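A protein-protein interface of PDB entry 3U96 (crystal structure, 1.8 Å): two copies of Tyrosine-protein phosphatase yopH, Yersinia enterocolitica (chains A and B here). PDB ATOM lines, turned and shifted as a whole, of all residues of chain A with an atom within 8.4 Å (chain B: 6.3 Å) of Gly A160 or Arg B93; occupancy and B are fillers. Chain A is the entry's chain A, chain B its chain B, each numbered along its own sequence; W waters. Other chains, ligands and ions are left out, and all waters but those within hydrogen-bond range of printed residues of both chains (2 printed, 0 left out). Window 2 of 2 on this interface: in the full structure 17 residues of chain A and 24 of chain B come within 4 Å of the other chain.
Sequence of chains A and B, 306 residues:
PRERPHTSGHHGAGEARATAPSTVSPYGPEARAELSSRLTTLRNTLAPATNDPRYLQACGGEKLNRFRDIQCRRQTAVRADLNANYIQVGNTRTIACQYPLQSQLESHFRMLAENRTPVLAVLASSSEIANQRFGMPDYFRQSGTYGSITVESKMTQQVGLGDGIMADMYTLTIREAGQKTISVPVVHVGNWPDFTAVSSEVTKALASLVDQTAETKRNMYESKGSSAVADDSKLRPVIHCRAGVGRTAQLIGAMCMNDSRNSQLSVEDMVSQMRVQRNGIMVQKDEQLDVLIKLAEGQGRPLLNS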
ATOM      1  N   GLN A 157       0.835 -27.183  33.255  1.00  0.00           N
ATOM      2  CA  GLN A 157       1.701 -26.596  32.230  1.00  0.00           C
ATOM      3  C   GLN A 157       2.557 -27.653  31.505  1.00  0.00           C
ATOM      4  O   GLN A 157       2.590 -28.821  31.916  1.00  0.00           O
ATOM      5  CB  GLN A 157       2.510 -25.385  32.783  1.00  0.00           C
ATOM      6  CG  GLN A 157       3.565 -25.681  33.804  1.00  0.00           C
ATOM      7  CD  GLN A 157       3.123 -25.466  35.252  1.00  0.00           C
ATOM      8  OE1 GLN A 157       3.895 -24.974  36.075  1.00  0.00           O
ATOM      9  NE2 GLN A 157       1.908 -25.878  35.580  1.00  0.00           N
ATOM     10  N   GLN A 158       3.170 -27.278  30.398  1.00  0.00           N
ATOM     11  CA  GLN A 158       4.166 -28.090  29.776  1.00  0.00           C
ATOM     12  C   GLN A 158       5.457 -27.275  29.634  1.00  0.00           C
ATOM     13  O   GLN A 158       5.387 -26.138  29.288  1.00  0.00           O
ATOM     14  CB  GLN A 158       3.674 -28.566  28.444  1.00  0.00           C
ATOM     15  CG  GLN A 158       4.526 -29.588  27.848  1.00  0.00           C
ATOM     16  CD  GLN A 158       4.181 -29.872  26.414  1.00  0.00           C
ATOM     17  OE1 GLN A 158       4.218 -28.990  25.574  1.00  0.00           O
ATOM     18  NE2 GLN A 158       3.848 -31.084  26.138  1.00  0.00           N
ATOM     19  N   VAL A 159       6.576 -27.868  29.997  1.00  0.00           N
ATOM     20  CA  VAL A 159       7.859 -27.153  30.045  1.00  0.00           C
ATOM     21  C   VAL A 159       8.885 -27.929  29.231  1.00  0.00           C
ATOM     22  O   VAL A 159       9.171 -29.102  29.541  1.00  0.00           O
ATOM     23  CB  VAL A 159       8.401 -26.961  31.498  1.00  0.00           C
ATOM     24  CG1 VAL A 159       9.816 -26.317  31.457  1.00  0.00           C
ATOM     25  CG2 VAL A 159       7.451 -26.088  32.370  1.00  0.00           C
ATOM     26  N   GLY A 160       9.480 -27.266  28.228  1.00  0.00           N
ATOM     27  CA  GLY A 160      10.527 -27.917  27.414  1.00  0.00           C
ATOM     28  C   GLY A 160      11.830 -27.970  28.212  1.00  0.00           C
ATOM     29  O   GLY A 160      12.173 -27.019  28.940  1.00  0.00           O
ATOM     30  N   LEU A 161      12.535 -29.085  28.113  1.00  0.00           N
ATOM     31  CA  LEU A 161      13.757 -29.275  28.877  1.00  0.00           C
ATOM     32  C   LEU A 161      15.037 -29.224  28.050  1.00  0.00           C
ATOM     33  O   LEU A 161      16.149 -29.270  28.609  1.00  0.00           O
ATOM     34  CB  LEU A 161      13.697 -30.599  29.650  1.00  0.00           C
ATOM     35  CG  LEU A 161      12.527 -30.822  30.620  1.00  0.00           C
ATOM     36  CD1 LEU A 161      12.507 -32.269  31.041  1.00  0.00           C
ATOM     37  CD2 LEU A 161      12.653 -29.937  31.869  1.00  0.00           C
ATOM     38  N   GLY A 162      14.873 -29.138  26.728  1.00  0.00           N
ATOM     39  CA  GLY A 162      15.998 -29.200  25.780  1.00  0.00           C
ATOM     40  C   GLY A 162      15.968 -30.495  24.975  1.00  0.00           C
ATOM     41  O   GLY A 162      15.374 -31.496  25.404  1.00  0.00           O
ATOM     42  N   ASP A 163      16.572 -30.465  23.784  1.00  0.00           N
ATOM     43  CA  ASP A 163      16.711 -31.657  22.939  1.00  0.00           C
ATOM     44  C   ASP A 163      15.347 -32.247  22.592  1.00  0.00           C
ATOM     45  O   ASP A 163      15.230 -33.444  22.319  1.00  0.00           O
ATOM     46  CB  ASP A 163      17.597 -32.712  23.641  1.00  0.00           C
ATOM     47  CG  ASP A 163      19.079 -32.357  23.642  1.00  0.00           C
ATOM     48  OD1 ASP A 163      19.838 -33.107  24.312  1.00  0.00           O
ATOM     49  OD2 ASP A 163      19.494 -31.349  22.996  1.00  0.00           O
ATOM     50  N   GLY A 164      14.312 -31.402  22.645  1.00  0.00           N
ATOM     51  CA  GLY A 164      12.940 -31.808  22.349  1.00  0.00           C
ATOM     52  C   GLY A 164      12.275 -32.654  23.441  1.00  0.00           C
ATOM     53  O   GLY A 164      11.140 -33.065  23.292  1.00  0.00           O
ATOM     54  N   ILE A 165      12.988 -32.891  24.538  1.00  0.00           N
ATOM     55  CA  ILE A 165      12.416 -33.602  25.713  1.00  0.00           C
ATOM     56  C   ILE A 165      11.424 -32.658  26.421  1.00  0.00           C
ATOM     57  O   ILE A 165      11.754 -31.486  26.646  1.00  0.00           O
ATOM     58  CB  ILE A 165      13.550 -34.046  26.689  1.00  0.00           C
ATOM     59  CG1 ILE A 165      14.620 -34.880  25.961  1.00  0.00           C
ATOM     60  CG2 ILE A 165      12.995 -34.812  27.895  1.00  0.00           C
ATOM     61  CD1 ILE A 165      14.048 -36.047  25.195  1.00  0.00           C
ATOM     62  N   MET A 166      10.232 -33.154  26.761  1.00  0.00           N
ATOM     63  CA  MET A 166       9.169 -32.302  27.316  1.00  0.00           C
ATOM     64  C   MET A 166       8.706 -32.828  28.669  1.00  0.00           C
ATOM     65  O   MET A 166       8.495 -34.035  28.840  1.00  0.00           O
ATOM     66  CB  MET A 166       7.947 -32.248  26.390  1.00  0.00           C
ATOM     67  CG  MET A 166       8.243 -31.839  24.942  1.00  0.00           C
ATOM     68  SD  MET A 166       8.888 -30.149  24.867  1.00  0.00           S
ATOM     69  CE  MET A 166       7.542 -29.290  25.632  1.00  0.00           C
ATOM     70  N   ALA A 167       8.537 -31.909  29.610  1.00  0.00           N
ATOM     71  CA  ALA A 167       7.888 -32.206  30.877  1.00  0.00           C
ATOM     72  C   ALA A 167       6.411 -31.827  30.811  1.00  0.00           C
ATOM     73  O   ALA A 167       6.055 -30.651  30.616  1.00  0.00           O
ATOM     74  CB  ALA A 167       8.582 -31.461  32.006  1.00  0.00           C
ATOM     75  N   ASP A 168       5.542 -32.822  30.941  1.00  0.00           N
ATOM     76  CA  ASP A 168       4.110 -32.566  31.030  1.00  0.00           C
ATOM     77  C   ASP A 168       3.725 -32.542  32.496  1.00  0.00           C
ATOM     78  O   ASP A 168       4.008 -33.481  33.221  1.00  0.00           O
ATOM     79  CB  ASP A 168       3.304 -33.653  30.321  1.00  0.00           C
ATOM     80  CG  ASP A 168       3.655 -33.798  28.859  1.00  0.00           C
ATOM     81  OD1 ASP A 168       3.830 -32.777  28.148  1.00  0.00           O
ATOM     82  OD2 ASP A 168       3.740 -34.959  28.407  1.00  0.00           O
ATOM     83  N   ASN A 191       8.369 -38.090  27.061  1.00  0.00           N
ATOM     84  CA  ASN A 191       9.169 -38.602  25.937  1.00  0.00           C
ATOM     85  C   ASN A 191      10.633 -38.825  26.329  1.00  0.00           C
ATOM     86  O   ASN A 191      11.544 -38.536  25.553  1.00  0.00           O
ATOM     87  CB  ASN A 191       9.035 -37.691  24.703  1.00  0.00           C
ATOM     88  CG  ASN A 191       9.575 -36.279  24.934  1.00  0.00           C
ATOM     89  OD1 ASN A 191       9.766 -35.827  26.084  1.00  0.00           O
ATOM     90  ND2 ASN A 191       9.861 -35.579  23.828  1.00  0.00           N
ATOM     91  N   GLU A 201      22.700 -31.558  30.311  1.00  0.00           N
ATOM     92  CA  GLU A 201      21.979 -30.282  30.191  1.00  0.00           C
ATOM     93  C   GLU A 201      20.470 -30.420  30.441  1.00  0.00           C
ATOM     94  O   GLU A 201      19.876 -29.603  31.141  1.00  0.00           O
ATOM     95  CB  GLU A 201      22.225 -29.642  28.812  1.00  0.00           C
ATOM     96  CG  GLU A 201      23.710 -29.216  28.580  1.00  0.00           C
ATOM     97  CD  GLU A 201      24.648 -30.327  28.046  1.00  0.00           C
ATOM     98  OE1 GLU A 201      24.211 -31.480  27.839  1.00  0.00           O
ATOM     99  OE2 GLU A 201      25.867 -30.038  27.868  1.00  0.00           O
ATOM    100  N   VAL A 202      19.865 -31.445  29.849  1.00  0.00           N
ATOM    101  CA  VAL A 202      18.454 -31.746  30.020  1.00  0.00           C
ATOM    102  C   VAL A 202      18.244 -32.194  31.481  1.00  0.00           C
ATOM    103  O   VAL A 202      17.289 -31.782  32.127  1.00  0.00           O
ATOM    104  CB  VAL A 202      17.992 -32.838  29.018  1.00  0.00           C
ATOM    105  CG1 VAL A 202      16.586 -33.334  29.361  1.00  0.00           C
ATOM    106  CG2 VAL A 202      17.961 -32.271  27.583  1.00  0.00           C
ATOM    107  N   ALA A 205      18.187 -29.185  33.643  1.00  0.00           N
ATOM    108  CA  ALA A 205      16.920 -28.444  33.448  1.00  0.00           C
ATOM    109  C   ALA A 205      15.749 -29.156  34.176  1.00  0.00           C
ATOM    110  O   ALA A 205      14.873 -28.515  34.734  1.00  0.00           O
ATOM    111  CB  ALA A 205      16.604 -28.282  31.949  1.00  0.00           C
ATOM    112  N   LEU A 206      15.758 -30.485  34.154  1.00  0.00           N
ATOM    113  CA  LEU A 206      14.733 -31.255  34.812  1.00  0.00           C
ATOM    114  C   LEU A 206      14.877 -31.144  36.329  1.00  0.00           C
ATOM    115  O   LEU A 206      13.891 -30.949  36.996  1.00  0.00           O
ATOM    116  CB  LEU A 206      14.824 -32.730  34.384  1.00  0.00           C
ATOM    117  CG  LEU A 206      13.832 -33.676  35.053  1.00  0.00           C
ATOM    118  CD1 LEU A 206      12.396 -33.263  34.733  1.00  0.00           C
ATOM    119  CD2 LEU A 206      14.116 -35.127  34.581  1.00  0.00           C
ATOM    120  N   LEU A 209      13.451 -27.778  37.355  1.00  0.00           N
ATOM    121  CA  LEU A 209      11.991 -27.788  37.298  1.00  0.00           C
ATOM    122  C   LEU A 209      11.371 -28.565  38.477  1.00  0.00           C
ATOM    123  O   LEU A 209      10.485 -28.071  39.141  1.00  0.00           O
ATOM    124  CB  LEU A 209      11.508 -28.394  35.985  1.00  0.00           C
ATOM    125  CG  LEU A 209      10.013 -28.632  35.901  1.00  0.00           C
ATOM    126  CD1 LEU A 209       9.234 -27.297  36.044  1.00  0.00           C
ATOM    127  CD2 LEU A 209       9.684 -29.350  34.581  1.00  0.00           C
ATOM    128  N   ILE B  87      16.595 -16.272  35.031  1.00  0.00           N
ATOM    129  CA  ILE B  87      15.285 -16.606  35.565  1.00  0.00           C
ATOM    130  C   ILE B  87      14.550 -17.294  34.444  1.00  0.00           C
ATOM    131  O   ILE B  87      14.553 -16.810  33.313  1.00  0.00           O
ATOM    132  CB  ILE B  87      14.470 -15.333  36.019  1.00  0.00           C
ATOM    133  CG1 ILE B  87      15.192 -14.603  37.175  1.00  0.00           C
ATOM    134  CG2 ILE B  87      13.047 -15.746  36.498  1.00  0.00           C
ATOM    135  CD1 ILE B  87      14.437 -13.412  37.725  1.00  0.00           C
ATOM    136  N   GLN B  88      13.953 -18.450  34.749  1.00  0.00           N
ATOM    137  CA  GLN B  88      13.011 -19.072  33.839  1.00  0.00           C
ATOM    138  C   GLN B  88      11.664 -19.170  34.492  1.00  0.00           C
ATOM    139  O   GLN B  88      11.515 -19.774  35.577  1.00  0.00           O
ATOM    140  CB  GLN B  88      13.492 -20.468  33.397  1.00  0.00           C
ATOM    141  CG  GLN B  88      12.600 -21.120  32.340  1.00  0.00           C
ATOM    142  CD  GLN B  88      13.180 -22.437  31.856  1.00  0.00           C
ATOM    143  OE1 GLN B  88      14.405 -22.604  31.817  1.00  0.00           O
ATOM    144  NE2 GLN B  88      12.316 -23.375  31.488  1.00  0.00           N
ATOM    145  N   VAL B  89      10.674 -18.584  33.835  1.00  0.00           N
ATOM    146  CA  VAL B  89       9.314 -18.586  34.362  1.00  0.00           C
ATOM    147  C   VAL B  89       8.477 -19.396  33.388  1.00  0.00           C
ATOM    148  O   VAL B  89       8.256 -18.974  32.233  1.00  0.00           O
ATOM    149  CB  VAL B  89       8.776 -17.151  34.536  1.00  0.00           C
ATOM    150  CG1 VAL B  89       7.345 -17.185  34.937  1.00  0.00           C
ATOM    151  CG2 VAL B  89       9.570 -16.411  35.612  1.00  0.00           C
ATOM    152  N   GLY B  90       8.058 -20.589  33.818  1.00  0.00           N
ATOM    153  CA  GLY B  90       7.464 -21.542  32.868  1.00  0.00           C
ATOM    154  C   GLY B  90       8.552 -21.899  31.861  1.00  0.00           C
ATOM    155  O   GLY B  90       9.593 -22.455  32.232  1.00  0.00           O
ATOM    156  N   ASN B  91       8.330 -21.537  30.594  1.00  0.00           N
ATOM    157  CA  ASN B  91       9.304 -21.762  29.543  1.00  0.00           C
ATOM    158  C   ASN B  91      10.140 -20.514  29.218  1.00  0.00           C
ATOM    159  O   ASN B  91      11.082 -20.578  28.428  1.00  0.00           O
ATOM    160  CB  ASN B  91       8.581 -22.176  28.267  1.00  0.00           C
ATOM    161  CG  ASN B  91       7.967 -23.559  28.361  1.00  0.00           C
ATOM    162  OD1 ASN B  91       8.661 -24.538  28.187  1.00  0.00           O
ATOM    163  ND2 ASN B  91       6.676 -23.630  28.655  1.00  0.00           N
ATOM    164  N   THR B  92       9.770 -19.374  29.791  1.00  0.00           N
ATOM    165  CA  THR B  92      10.374 -18.091  29.392  1.00  0.00           C
ATOM    166  C   THR B  92      11.724 -17.849  30.063  1.00  0.00           C
ATOM    167  O   THR B  92      11.798 -17.758  31.307  1.00  0.00           O
ATOM    168  CB  THR B  92       9.414 -16.958  29.758  1.00  0.00           C
ATOM    169  OG1 THR B  92       8.127 -17.257  29.202  1.00  0.00           O
ATOM    170  CG2 THR B  92       9.902 -15.605  29.187  1.00  0.00           C
ATOM    171  N   ARG B  93      12.785 -17.707  29.258  1.00  0.00           N
ATOM    172  CA  ARG B  93      14.126 -17.546  29.836  1.00  0.00           C
ATOM    173  C   ARG B  93      14.596 -16.110  29.688  1.00  0.00           C
ATOM    174  O   ARG B  93      14.587 -15.566  28.590  1.00  0.00           O
ATOM    175  CB  ARG B  93      15.153 -18.479  29.195  1.00  0.00           C
ATOM    176  CG  ARG B  93      14.874 -19.968  29.424  1.00  0.00           C
ATOM    177  CD  ARG B  93      15.493 -20.793  28.275  1.00  0.00           C
ATOM    178  NE  ARG B  93      15.338 -22.244  28.460  1.00  0.00           N
ATOM    179  CZ  ARG B  93      14.256 -22.973  28.148  1.00  0.00           C
ATOM    180  NH1 ARG B  93      13.147 -22.430  27.633  1.00  0.00           N
ATOM    181  NH2 ARG B  93      14.299 -24.281  28.348  1.00  0.00           N
ATOM    182  N   THR B  94      14.981 -15.515  30.810  1.00  0.00           N
ATOM    183  CA  THR B  94      15.417 -14.125  30.841  1.00  0.00           C
ATOM    184  C   THR B  94      16.609 -13.986  31.770  1.00  0.00           C
ATOM    185  O   THR B  94      17.044 -14.957  32.418  1.00  0.00           O
ATOM    186  CB  THR B  94      14.295 -13.146  31.324  1.00  0.00           C
ATOM    187  OG1 THR B  94      13.938 -13.404  32.693  1.00  0.00           O
ATOM    188  CG2 THR B  94      13.037 -13.229  30.420  1.00  0.00           C
ATOM    189  N   ILE B  95      17.092 -12.752  31.878  1.00  0.00           N
ATOM    190  CA  ILE B  95      18.045 -12.382  32.899  1.00  0.00           C
ATOM    191  C   ILE B  95      17.479 -11.121  33.521  1.00  0.00           C
ATOM    192  O   ILE B  95      17.048 -10.216  32.793  1.00  0.00           O
ATOM    193  CB  ILE B  95      19.449 -12.063  32.295  1.00  0.00           C
ATOM    194  CG1 ILE B  95      20.160 -13.367  31.880  1.00  0.00           C
ATOM    195  CG2 ILE B  95      20.313 -11.291  33.340  1.00  0.00           C
ATOM    196  CD1 ILE B  95      21.413 -13.116  30.992  1.00  0.00           C
ATOM    197  N   ASP B 232      21.423 -22.742  26.437  1.00  0.00           N
ATOM    198  CA  ASP B 232      20.327 -22.287  27.297  1.00  0.00           C
ATOM    199  C   ASP B 232      20.629 -21.070  28.169  1.00  0.00           C
ATOM    200  O   ASP B 232      19.706 -20.376  28.621  1.00  0.00           O
ATOM    201  CB  ASP B 232      19.792 -23.437  28.160  1.00  0.00           C
ATOM    202  CG  ASP B 232      18.610 -24.126  27.526  1.00  0.00           C
ATOM    203  OD1 ASP B 232      17.612 -23.433  27.187  1.00  0.00           O
ATOM    204  OD2 ASP B 232      18.669 -25.367  27.367  1.00  0.00           O
ATOM    205  N   LYS B 234      22.252 -18.574  26.947  1.00  0.00           N
ATOM    206  CA  LYS B 234      22.418 -17.439  26.001  1.00  0.00           C
ATOM    207  C   LYS B 234      21.131 -17.028  25.271  1.00  0.00           C
ATOM    208  O   LYS B 234      20.112 -17.707  25.368  1.00  0.00           O
ATOM    209  CB  LYS B 234      23.546 -17.742  24.996  1.00  0.00           C
ATOM    210  CG  LYS B 234      24.903 -17.829  25.691  1.00  0.00           C
ATOM    211  CD  LYS B 234      26.042 -18.081  24.715  1.00  0.00           C
ATOM    212  CE  LYS B 234      27.308 -18.556  25.458  1.00  0.00           C
ATOM    213  NZ  LYS B 234      27.864 -17.497  26.325  1.00  0.00           N
ATOM    214  N   LEU B 235      21.199 -15.906  24.545  1.00  0.00           N
ATOM    215  CA  LEU B 235      20.036 -15.312  23.858  1.00  0.00           C
ATOM    216  C   LEU B 235      18.874 -14.931  24.790  1.00  0.00           C
ATOM    217  O   LEU B 235      17.713 -14.926  24.389  1.00  0.00           O
ATOM    218  CB  LEU B 235      19.553 -16.187  22.669  1.00  0.00           C
ATOM    219  CG  LEU B 235      20.533 -16.246  21.488  1.00  0.00           C
ATOM    220  CD1 LEU B 235      20.125 -17.331  20.472  1.00  0.00           C
ATOM    221  CD2 LEU B 235      20.700 -14.923  20.813  1.00  0.00           C
ATOM    222  N   ARG B 236      19.191 -14.566  26.029  1.00  0.00           N
ATOM    223  CA  ARG B 236      18.150 -14.172  26.966  1.00  0.00           C
ATOM    224  C   ARG B 236      17.922 -12.672  26.921  1.00  0.00           C
ATOM    225  O   ARG B 236      18.865 -11.926  26.997  1.00  0.00           O
ATOM    226  CB  ARG B 236      18.515 -14.577  28.377  1.00  0.00           C
ATOM    227  CG  ARG B 236      18.621 -16.115  28.530  1.00  0.00           C
ATOM    228  CD  ARG B 236      19.024 -16.490  29.917  1.00  0.00           C
ATOM    229  NE  ARG B 236      18.959 -17.960  30.081  1.00  0.00           N
ATOM    230  CZ  ARG B 236      18.232 -18.591  30.998  1.00  0.00           C
ATOM    231  NH1 ARG B 236      17.499 -17.903  31.870  1.00  0.00           N
ATOM    232  NH2 ARG B 236      18.270 -19.921  31.055  1.00  0.00           N
ATOM    233  N   PRO B 237      16.659 -12.247  26.829  1.00  0.00           N
ATOM    234  CA  PRO B 237      16.371 -10.826  27.110  1.00  0.00           C
ATOM    235  C   PRO B 237      16.870 -10.470  28.511  1.00  0.00           C
ATOM    236  O   PRO B 237      16.713 -11.274  29.461  1.00  0.00           O
ATOM    237  CB  PRO B 237      14.831 -10.771  27.064  1.00  0.00           C
ATOM    238  CG  PRO B 237      14.440 -11.940  26.197  1.00  0.00           C
ATOM    239  CD  PRO B 237      15.420 -13.013  26.591  1.00  0.00           C
ATOM    240  N   ASP B 259       3.961 -15.523  26.309  1.00  0.00           N
ATOM    241  CA  ASP B 259       4.632 -16.706  25.755  1.00  0.00           C
ATOM    242  C   ASP B 259       3.582 -17.814  25.599  1.00  0.00           C
ATOM    243  O   ASP B 259       2.982 -18.271  26.601  1.00  0.00           O
ATOM    244  CB  ASP B 259       5.761 -17.137  26.710  1.00  0.00           C
ATOM    245  CG  ASP B 259       6.653 -18.249  26.150  1.00  0.00           C
ATOM    246  OD1 ASP B 259       6.203 -19.073  25.310  1.00  0.00           O
ATOM    247  OD2 ASP B 259       7.830 -18.309  26.590  1.00  0.00           O
ATOM    248  N   ARG B 261       3.833 -20.792  25.151  1.00  0.00           N
ATOM    249  CA  ARG B 261       4.186 -22.099  25.705  1.00  0.00           C
ATOM    250  C   ARG B 261       3.713 -22.249  27.163  1.00  0.00           C
ATOM    251  O   ARG B 261       3.739 -23.350  27.703  1.00  0.00           O
ATOM    252  CB  ARG B 261       5.697 -22.344  25.599  1.00  0.00           C
ATOM    253  CG  ARG B 261       6.259 -22.237  24.154  1.00  0.00           C
ATOM    254  CD  ARG B 261       7.776 -22.221  24.111  1.00  0.00           C
ATOM    255  NE  ARG B 261       8.333 -20.971  24.633  1.00  0.00           N
ATOM    256  CZ  ARG B 261       9.620 -20.784  24.922  1.00  0.00           C
ATOM    257  NH1 ARG B 261      10.506 -21.753  24.731  1.00  0.00           N
ATOM    258  NH2 ARG B 261      10.034 -19.624  25.408  1.00  0.00           N
HETATM  259  O   HOH W   1      13.573 -25.860  30.874  1.00  0.00           O
HETATM  260  O   HOH W   2       2.198 -24.856  29.320  1.00  0.00           O
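Of chain B, only Asn B91 (2.8 Å) and Arg B93 (3.5 Å) come within 4 Å of Gly A160. Of chain A, only Gly A160 (3.5 Å) comes within 4 Å of Arg B93. Of the printed residues of chain A, Gly B90 touches Val A159 (3.9 Å). Printed residues of chain B within 4 Å of Val A159: Gln B88 (3.9 Å), Gly B90 (3.9 Å) and Asn B91 (3.3 Å). The nearest residue of chain B that does not touch Gly A160 is Gln B88 (4.4 Å). The nearest residue of chain A that does not touch Arg B93 is Leu A161 (5.0 Å).
The side-chain carboxylate (OD1) of Asp A168 is in hydrogen-bond range of the side-chain amide nitrogen (NE2) of Gln A158 (2.6 Å). The side-chain amide nitrogen (NE2) of Gln B88 lies within hydrogen-bond range of the backbone carbonyl oxygen (O) of Gly B90 (3.0 Å). The guanidinium group (NH1) of Arg B93 lies within hydrogen-bond range of the backbone carbonyl oxygen (O) of Asn B91, 2.9 Å away. The side-chain amide nitrogen (ND2) of Asn B91 sits at hydrogen-bond distance from the backbone carbonyl oxygen (O) of Arg B261, at 3.1 Å. The side-chain carboxylate (OD1) of Asp B232 lies within salt-bridge range of the guanidinium group (NE) of Arg B93 (2.9 Å). The side-chain carboxylate (OD2) of Asp B259 is in salt-bridge range of the guanidinium group (NH2) of Arg B261 (2.8 Å).
The side-chain amide nitrogen of Asn B91 sits at hydrogen-bond distance from the backbone carbonyl oxygen of Gln A158 (2.9 Å). OD1 of Asn B91 is in hydrogen-bond range of N of Gly A160 (2.8 Å).
Among the printed residues, pairs that only touch across the chains: Val A159 with Asn B91 (3.3 Å), Gly A160 with Arg B93 (3.5 Å), Gln A158 with Arg B261 (3.6 Å), Val A159 with Gln B88 (3.9 Å) and Val A159 with Gly B90 (3.9 Å).
No position is printed for both chains.
Printed residues of chain A that touch a printed residue of chain B: Gln A158, Val A159 and Gly A160. Hydrophobic or aromatic side chains of chain A that line the printed part of chain B: Val A159. Among the printed residues, 7 pairs touch across the chains.
Water W1 lies within hydrogen-bond range of O of Gly A160 (2.7 Å), NE2 of Gln B88 (2.9 Å) and NH2 of Arg B93 (3.1 Å). Water W2 bridges the backbone carbonyl oxygen of Arg B261 (2.7 Å) and the backbone NH of Gln A158 (2.8 Å).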
